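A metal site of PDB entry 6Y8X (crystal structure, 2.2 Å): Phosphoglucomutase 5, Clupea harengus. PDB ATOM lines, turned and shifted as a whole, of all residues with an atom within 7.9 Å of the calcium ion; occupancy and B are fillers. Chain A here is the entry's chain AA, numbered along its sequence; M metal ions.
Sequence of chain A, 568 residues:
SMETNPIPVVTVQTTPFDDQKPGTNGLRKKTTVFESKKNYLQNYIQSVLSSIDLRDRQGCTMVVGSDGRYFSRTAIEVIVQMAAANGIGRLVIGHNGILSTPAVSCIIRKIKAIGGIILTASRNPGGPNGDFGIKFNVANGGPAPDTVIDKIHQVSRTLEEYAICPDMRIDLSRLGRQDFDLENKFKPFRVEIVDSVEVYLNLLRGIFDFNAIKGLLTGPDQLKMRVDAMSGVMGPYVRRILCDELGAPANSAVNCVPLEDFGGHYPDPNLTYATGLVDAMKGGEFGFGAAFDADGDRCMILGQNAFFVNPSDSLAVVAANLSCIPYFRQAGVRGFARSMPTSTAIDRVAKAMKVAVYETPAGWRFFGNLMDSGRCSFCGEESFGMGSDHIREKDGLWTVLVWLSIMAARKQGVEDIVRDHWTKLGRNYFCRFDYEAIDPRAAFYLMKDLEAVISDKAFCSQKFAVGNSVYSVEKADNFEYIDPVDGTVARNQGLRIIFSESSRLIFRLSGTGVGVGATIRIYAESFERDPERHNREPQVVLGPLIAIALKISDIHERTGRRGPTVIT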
ATOM      1  N   ASN A  25     -12.644   8.043  11.170  1.00  0.00           N
ATOM      2  CA  ASN A  25     -12.854   9.418  11.606  1.00  0.00           C
ATOM      3  C   ASN A  25     -13.453  10.250  10.485  1.00  0.00           C
ATOM      4  O   ASN A  25     -12.903  11.300  10.119  1.00  0.00           O
ATOM      5  CB  ASN A  25     -11.545  10.021  12.112  1.00  0.00           C
ATOM      6  CG  ASN A  25     -10.356   9.647  11.250  1.00  0.00           C
ATOM      7  OD1 ASN A  25     -10.422   9.711  10.017  1.00  0.00           O
ATOM      8  ND2 ASN A  25      -9.265   9.235  11.883  1.00  0.00           N
ATOM      9  N   ARG A  28     -12.869  12.214   4.669  1.00  0.00           N
ATOM     10  CA  ARG A  28     -11.872  13.261   4.480  1.00  0.00           C
ATOM     11  C   ARG A  28     -11.456  13.331   3.023  1.00  0.00           C
ATOM     12  O   ARG A  28     -10.998  12.329   2.458  1.00  0.00           O
ATOM     13  CB  ARG A  28     -10.639  13.020   5.348  1.00  0.00           C
ATOM     14  CG  ARG A  28     -10.880  13.064   6.849  1.00  0.00           C
ATOM     15  CD  ARG A  28      -9.560  12.928   7.588  1.00  0.00           C
ATOM     16  NE  ARG A  28      -9.718  12.763   9.024  1.00  0.00           N
ATOM     17  CZ  ARG A  28      -8.721  12.535   9.868  1.00  0.00           C
ATOM     18  NH1 ARG A  28      -7.472  12.446   9.412  1.00  0.00           N
ATOM     19  NH2 ARG A  28      -8.963  12.397  11.164  1.00  0.00           N
ATOM     20  N   ASP A  67     -14.728  23.081  13.000  1.00  0.00           N
ATOM     21  CA  ASP A  67     -13.496  23.569  13.592  1.00  0.00           C
ATOM     22  C   ASP A  67     -13.073  24.915  13.024  1.00  0.00           C
ATOM     23  O   ASP A  67     -11.994  25.416  13.362  1.00  0.00           O
ATOM     24  CB  ASP A  67     -12.365  22.546  13.384  1.00  0.00           C
ATOM     25  CG  ASP A  67     -12.118  22.217  11.925  1.00  0.00           C
ATOM     26  OD1 ASP A  67     -12.578  22.986  11.047  1.00  0.00           O
ATOM     27  OD2 ASP A  67     -11.452  21.195  11.645  1.00  0.00           O
ATOM     28  N   THR A 101     -15.667  18.958  18.758  1.00  0.00           N
ATOM     29  CA  THR A 101     -16.213  17.600  18.797  1.00  0.00           C
ATOM     30  C   THR A 101     -16.659  17.183  20.184  1.00  0.00           C
ATOM     31  O   THR A 101     -17.749  16.611  20.311  1.00  0.00           O
ATOM     32  CB  THR A 101     -15.181  16.619  18.228  1.00  0.00           C
ATOM     33  OG1 THR A 101     -15.018  16.871  16.827  1.00  0.00           O
ATOM     34  CG2 THR A 101     -15.615  15.177  18.418  1.00  0.00           C
ATOM     35  N   PRO A 102     -15.891  17.423  21.259  1.00  0.00           N
ATOM     36  CA  PRO A 102     -16.418  17.103  22.593  1.00  0.00           C
ATOM     37  C   PRO A 102     -17.688  17.862  22.931  1.00  0.00           C
ATOM     38  O   PRO A 102     -18.617  17.289  23.502  1.00  0.00           O
ATOM     39  CB  PRO A 102     -15.252  17.481  23.527  1.00  0.00           C
ATOM     40  CG  PRO A 102     -14.037  17.454  22.659  1.00  0.00           C
ATOM     41  CD  PRO A 102     -14.506  17.912  21.321  1.00  0.00           C
ATOM     42  N   THR A 120     -14.909  18.816  10.170  1.00  0.00           N
ATOM     43  CA  THR A 120     -13.529  18.889  10.608  1.00  0.00           C
ATOM     44  C   THR A 120     -12.754  17.725   9.997  1.00  0.00           C
ATOM     45  O   THR A 120     -13.331  16.678   9.680  1.00  0.00           O
ATOM     46  CB  THR A 120     -13.420  18.847  12.140  1.00  0.00           C
ATOM     47  OG1 THR A 120     -12.044  18.960  12.526  1.00  0.00           O
ATOM     48  CG2 THR A 120     -13.977  17.540  12.681  1.00  0.00           C
ATOM     49  N   ALA A 121     -11.449  17.929   9.844  1.00  0.00           N
ATOM     50  CA  ALA A 121     -10.517  16.878   9.445  1.00  0.00           C
ATOM     51  C   ALA A 121      -9.507  16.576  10.539  1.00  0.00           C
ATOM     52  O   ALA A 121      -8.423  16.057  10.264  1.00  0.00           O
ATOM     53  CB  ALA A 121      -9.808  17.257   8.145  1.00  0.00           C
ATOM     54  N   SER A 122      -9.844  16.901  11.794  1.00  0.00           N
ATOM     55  CA  SER A 122      -9.000  16.617  12.945  1.00  0.00           C
ATOM     56  C   SER A 122      -7.587  17.152  12.768  1.00  0.00           C
ATOM     57  O   SER A 122      -7.332  18.342  13.008  1.00  0.00           O
ATOM     58  CB  SER A 122      -8.955  15.109  13.213  1.00  0.00           C
ATOM     59  OG  SER A 122     -10.213  14.637  13.664  1.00  0.00           O
ATOM     60  N   ARG A 123      -6.658  16.302  12.351  1.00  0.00           N
ATOM     61  CA  ARG A 123      -5.238  16.638  12.329  1.00  0.00           C
ATOM     62  C   ARG A 123      -4.779  17.177  10.988  1.00  0.00           C
ATOM     63  O   ARG A 123      -3.577  17.424  10.811  1.00  0.00           O
ATOM     64  CB  ARG A 123      -4.401  15.400  12.683  1.00  0.00           C
ATOM     65  CG  ARG A 123      -4.985  14.507  13.768  1.00  0.00           C
ATOM     66  CD  ARG A 123      -4.471  13.086  13.631  1.00  0.00           C
ATOM     67  NE  ARG A 123      -3.030  12.991  13.866  1.00  0.00           N
ATOM     68  CZ  ARG A 123      -2.249  12.020  13.415  1.00  0.00           C
ATOM     69  NH1 ARG A 123      -2.765  11.033  12.680  1.00  0.00           N
ATOM     70  NH2 ARG A 123      -0.956  12.023  13.684  1.00  0.00           N
ATOM     71  N   ASN A 124      -5.693  17.395  10.036  1.00  0.00           N
ATOM     72  CA  ASN A 124      -5.298  17.767   8.691  1.00  0.00           C
ATOM     73  C   ASN A 124      -5.372  19.270   8.494  1.00  0.00           C
ATOM     74  O   ASN A 124      -6.184  19.958   9.131  1.00  0.00           O
ATOM     75  CB  ASN A 124      -6.209  17.084   7.664  1.00  0.00           C
ATOM     76  CG  ASN A 124      -6.052  15.575   7.661  1.00  0.00           C
ATOM     77  OD1 ASN A 124      -5.370  15.012   8.521  1.00  0.00           O
ATOM     78  ND2 ASN A 124      -6.677  14.913   6.700  1.00  0.00           N
ATOM     79  N   LYS A 135     -17.703  14.404   9.844  1.00  0.00           N
ATOM     80  CA  LYS A 135     -17.941  13.353  10.812  1.00  0.00           C
ATOM     81  C   LYS A 135     -19.404  13.359  11.219  1.00  0.00           C
ATOM     82  O   LYS A 135     -20.023  14.420  11.312  1.00  0.00           O
ATOM     83  CB  LYS A 135     -17.041  13.519  12.039  1.00  0.00           C
ATOM     84  CG  LYS A 135     -15.637  12.935  11.848  1.00  0.00           C
ATOM     85  CD  LYS A 135     -14.560  13.700  12.620  1.00  0.00           C
ATOM     86  CE  LYS A 135     -14.407  13.211  14.055  1.00  0.00           C
ATOM     87  NZ  LYS A 135     -13.081  13.621  14.623  1.00  0.00           N
ATOM     88  N   PRO A 267      -2.620  20.913  12.438  1.00  0.00           N
ATOM     89  CA  PRO A 267      -3.133  20.767  13.818  1.00  0.00           C
ATOM     90  C   PRO A 267      -3.058  19.325  14.307  1.00  0.00           C
ATOM     91  O   PRO A 267      -4.077  18.703  14.644  1.00  0.00           O
ATOM     92  CB  PRO A 267      -4.569  21.278  13.681  1.00  0.00           C
ATOM     93  CG  PRO A 267      -4.980  20.827  12.301  1.00  0.00           C
ATOM     94  CD  PRO A 267      -3.716  20.841  11.444  1.00  0.00           C
ATOM     95  N   PRO A 269      -1.414  17.252  17.155  1.00  0.00           N
ATOM     96  CA  PRO A 269      -0.661  17.290  18.416  1.00  0.00           C
ATOM     97  C   PRO A 269       0.333  16.146  18.559  1.00  0.00           C
ATOM     98  O   PRO A 269      -0.043  14.997  18.776  1.00  0.00           O
ATOM     99  CB  PRO A 269      -1.761  17.193  19.488  1.00  0.00           C
ATOM    100  CG  PRO A 269      -2.999  17.664  18.805  1.00  0.00           C
ATOM    101  CD  PRO A 269      -2.865  17.211  17.382  1.00  0.00           C
ATOM    102  N   PHE A 292      -3.756  21.089  21.264  1.00  0.00           N
ATOM    103  CA  PHE A 292      -4.959  20.434  20.786  1.00  0.00           C
ATOM    104  C   PHE A 292      -4.939  20.337  19.266  1.00  0.00           C
ATOM    105  O   PHE A 292      -4.220  21.062  18.577  1.00  0.00           O
ATOM    106  CB  PHE A 292      -6.219  21.196  21.220  1.00  0.00           C
ATOM    107  CG  PHE A 292      -6.346  21.358  22.714  1.00  0.00           C
ATOM    108  CD1 PHE A 292      -6.452  20.253  23.532  1.00  0.00           C
ATOM    109  CD2 PHE A 292      -6.370  22.618  23.283  1.00  0.00           C
ATOM    110  CE1 PHE A 292      -6.576  20.399  24.900  1.00  0.00           C
ATOM    111  CE2 PHE A 292      -6.496  22.778  24.654  1.00  0.00           C
ATOM    112  CZ  PHE A 292      -6.591  21.661  25.466  1.00  0.00           C
ATOM    113  N   ASP A 293      -5.754  19.422  18.738  1.00  0.00           N
ATOM    114  CA  ASP A 293      -5.960  19.314  17.308  1.00  0.00           C
ATOM    115  C   ASP A 293      -7.095  20.239  16.875  1.00  0.00           C
ATOM    116  O   ASP A 293      -7.668  20.980  17.677  1.00  0.00           O
ATOM    117  CB  ASP A 293      -6.228  17.865  16.908  1.00  0.00           C
ATOM    118  CG  ASP A 293      -7.429  17.279  17.616  1.00  0.00           C
ATOM    119  OD1 ASP A 293      -8.033  17.997  18.441  1.00  0.00           O
ATOM    120  OD2 ASP A 293      -7.762  16.114  17.349  1.00  0.00           O
ATOM    121  N   ALA A 294      -7.426  20.194  15.586  1.00  0.00           N
ATOM    122  CA  ALA A 294      -8.350  21.187  15.025  1.00  0.00           C
ATOM    123  C   ALA A 294      -9.722  21.121  15.692  1.00  0.00           C
ATOM    124  O   ALA A 294     -10.330  22.160  15.961  1.00  0.00           O
ATOM    125  CB  ALA A 294      -8.488  20.981  13.516  1.00  0.00           C
ATOM    126  N   ASP A 295     -10.224  19.912  15.977  1.00  0.00           N
ATOM    127  CA  ASP A 295     -11.567  19.752  16.518  1.00  0.00           C
ATOM    128  C   ASP A 295     -11.582  19.616  18.043  1.00  0.00           C
ATOM    129  O   ASP A 295     -12.661  19.554  18.625  1.00  0.00           O
ATOM    130  CB  ASP A 295     -12.263  18.540  15.881  1.00  0.00           C
ATOM    131  CG  ASP A 295     -11.473  17.259  16.039  1.00  0.00           C
ATOM    132  OD1 ASP A 295     -10.226  17.327  16.145  1.00  0.00           O
ATOM    133  OD2 ASP A 295     -12.112  16.182  16.030  1.00  0.00           O
ATOM    134  N   GLY A 296     -10.416  19.559  18.692  1.00  0.00           N
ATOM    135  CA  GLY A 296     -10.347  19.619  20.134  1.00  0.00           C
ATOM    136  C   GLY A 296     -10.538  18.310  20.867  1.00  0.00           C
ATOM    137  O   GLY A 296     -10.836  18.339  22.066  1.00  0.00           O
ATOM    138  N   ASP A 297     -10.369  17.171  20.195  1.00  0.00           N
ATOM    139  CA  ASP A 297     -10.563  15.875  20.831  1.00  0.00           C
ATOM    140  C   ASP A 297      -9.248  15.175  21.166  1.00  0.00           C
ATOM    141  O   ASP A 297      -9.224  14.356  22.090  1.00  0.00           O
ATOM    142  CB  ASP A 297     -11.405  14.968  19.941  1.00  0.00           C
ATOM    143  CG  ASP A 297     -10.806  14.783  18.558  1.00  0.00           C
ATOM    144  OD1 ASP A 297     -10.088  15.698  18.106  1.00  0.00           O
ATOM    145  OD2 ASP A 297     -11.059  13.734  17.928  1.00  0.00           O
ATOM    146  N   ARG A 298      -8.175  15.457  20.439  1.00  0.00           N
ATOM    147  CA  ARG A 298      -6.847  14.924  20.751  1.00  0.00           C
ATOM    148  C   ARG A 298      -6.026  15.981  21.475  1.00  0.00           C
ATOM    149  O   ARG A 298      -6.277  17.180  21.371  1.00  0.00           O
ATOM    150  CB  ARG A 298      -6.141  14.484  19.469  1.00  0.00           C
ATOM    151  CG  ARG A 298      -6.811  13.315  18.746  1.00  0.00           C
ATOM    152  CD  ARG A 298      -6.060  12.968  17.463  1.00  0.00           C
ATOM    153  NE  ARG A 298      -6.446  11.658  16.923  1.00  0.00           N
ATOM    154  CZ  ARG A 298      -7.389  11.454  16.019  1.00  0.00           C
ATOM    155  NH1 ARG A 298      -8.098  12.473  15.535  1.00  0.00           N
ATOM    156  NH2 ARG A 298      -7.643  10.223  15.596  1.00  0.00           N
ATOM    157  N   CYS A 299      -5.026  15.512  22.217  1.00  0.00           N
ATOM    158  CA  CYS A 299      -4.269  16.415  23.078  1.00  0.00           C
ATOM    159  C   CYS A 299      -2.904  15.813  23.394  1.00  0.00           C
ATOM    160  O   CYS A 299      -2.819  14.648  23.819  1.00  0.00           O
ATOM    161  CB  CYS A 299      -5.032  16.691  24.377  1.00  0.00           C
ATOM    162  SG  CYS A 299      -4.125  17.655  25.588  1.00  0.00           S
ATOM    163  N   SER A 383      -3.206   7.280  20.284  1.00  0.00           N
ATOM    164  CA  SER A 383      -3.355   8.365  19.306  1.00  0.00           C
ATOM    165  C   SER A 383      -3.735   9.697  19.942  1.00  0.00           C
ATOM    166  O   SER A 383      -4.510  10.470  19.374  1.00  0.00           O
ATOM    167  CB  SER A 383      -4.398   7.945  18.265  1.00  0.00           C
ATOM    168  OG  SER A 383      -5.569   7.427  18.882  1.00  0.00           O
ATOM    169  N   PHE A 384      -3.182   9.998  21.115  1.00  0.00           N
ATOM    170  CA  PHE A 384      -3.407  11.274  21.799  1.00  0.00           C
ATOM    171  C   PHE A 384      -4.872  11.473  22.155  1.00  0.00           C
ATOM    172  O   PHE A 384      -5.382  12.601  22.165  1.00  0.00           O
ATOM    173  CB  PHE A 384      -2.885  12.439  20.943  1.00  0.00           C
ATOM    174  CG  PHE A 384      -1.410  12.365  20.657  1.00  0.00           C
ATOM    175  CD1 PHE A 384      -0.921  11.495  19.690  1.00  0.00           C
ATOM    176  CD2 PHE A 384      -0.507  13.143  21.367  1.00  0.00           C
ATOM    177  CE1 PHE A 384       0.445  11.417  19.429  1.00  0.00           C
ATOM    178  CE2 PHE A 384       0.847  13.071  21.103  1.00  0.00           C
ATOM    179  CZ  PHE A 384       1.325  12.213  20.142  1.00  0.00           C
ATOM    180  N   GLU A 393     -17.011  10.769  23.360  1.00  0.00           N
ATOM    181  CA  GLU A 393     -15.910  11.125  22.475  1.00  0.00           C
ATOM    182  C   GLU A 393     -14.668  11.381  23.308  1.00  0.00           C
ATOM    183  O   GLU A 393     -14.745  11.623  24.522  1.00  0.00           O
ATOM    184  CB  GLU A 393     -16.237  12.376  21.636  1.00  0.00           C
ATOM    185  CG  GLU A 393     -16.984  12.097  20.348  1.00  0.00           C
ATOM    186  CD  GLU A 393     -16.059  11.667  19.215  1.00  0.00           C
ATOM    187  OE1 GLU A 393     -14.850  11.474  19.467  1.00  0.00           O
ATOM    188  OE2 GLU A 393     -16.540  11.537  18.067  1.00  0.00           O
ATOM    189  N   LYS A 394     -13.513  11.315  22.654  1.00  0.00           N
ATOM    190  CA  LYS A 394     -12.275  11.750  23.296  1.00  0.00           C
ATOM    191  C   LYS A 394     -12.299  13.267  23.442  1.00  0.00           C
ATOM    192  O   LYS A 394     -12.764  13.993  22.559  1.00  0.00           O
ATOM    193  CB  LYS A 394     -11.059  11.312  22.474  1.00  0.00           C
ATOM    194  CG  LYS A 394     -11.281  11.185  20.986  1.00  0.00           C
ATOM    195  CD  LYS A 394      -9.998  10.864  20.242  1.00  0.00           C
ATOM    196  CE  LYS A 394     -10.258  10.627  18.765  1.00  0.00           C
ATOM    197  NZ  LYS A 394      -9.122   9.948  18.108  1.00  0.00           N
HETATM  198 CA    CA M   1      -9.554  15.013  15.985  1.00  0.00          CA
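The side-chain carboxylate (OD1) of Asp 293 sits at hydrogen-bond distance from the backbone NH (N) of Arg 298. The side-chain carboxylate (OD1) of Asp 293 sits at hydrogen-bond distance from the backbone NH (N) of Gly 296 (2.9 Å). The guanidinium group (NE) of Arg 298 lies within hydrogen-bond range of the backbone carbonyl oxygen (O) of Ser 383 (3.3 Å). The backbone NH (N) of Ser 122 lies within hydrogen-bond range of the side-chain hydroxyl (OG1) of Thr 120. The side-chain hydroxyl (OG) of Ser 122 lies close to the side-chain amino group (NZ) of Lys 135 (3.2 Å). The side-chain carboxylate of Asp 297 lies close to the side-chain amino group of Lys 135, 3.9 Å away. The backbone carbonyl oxygen (O) of Asp 295 sits at hydrogen-bond distance from the backbone NH (N) of Thr 101 (3.1 Å). The backbone carbonyl oxygen (O) of Ser 122 sits close to the backbone NH (N) of Ala 294 (3.2 Å).
Five residues have an atom within 4 Å of the calcium ion: Ser 122, Asp 293, Asp 295, Asp 297 and Arg 298. The nearest printed residue that does not touch the calcium ion is Lys 135 (4.03 Å).
The calcium ion is bound by the side-chain carboxylate (OD1) of Asp 297 (2.3 Å), the side-chain carboxylate (OD1) of Asp 295 (2.4 Å), the side-chain hydroxyl (OG) of Ser 122 (2.4 Å), the side-chain carboxylate (OD2) of Asp 293 (2.5 Å), the side-chain carboxylate (OD2) of Asp 297 (2.8 Å) and the side-chain carboxylate (OD2) of Asp 295 (2.8 Å). The calcium ion has six donor atoms within binding distance. Slightly farther from the calcium ion lies NH1 of Arg 298 (3.0 Å).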
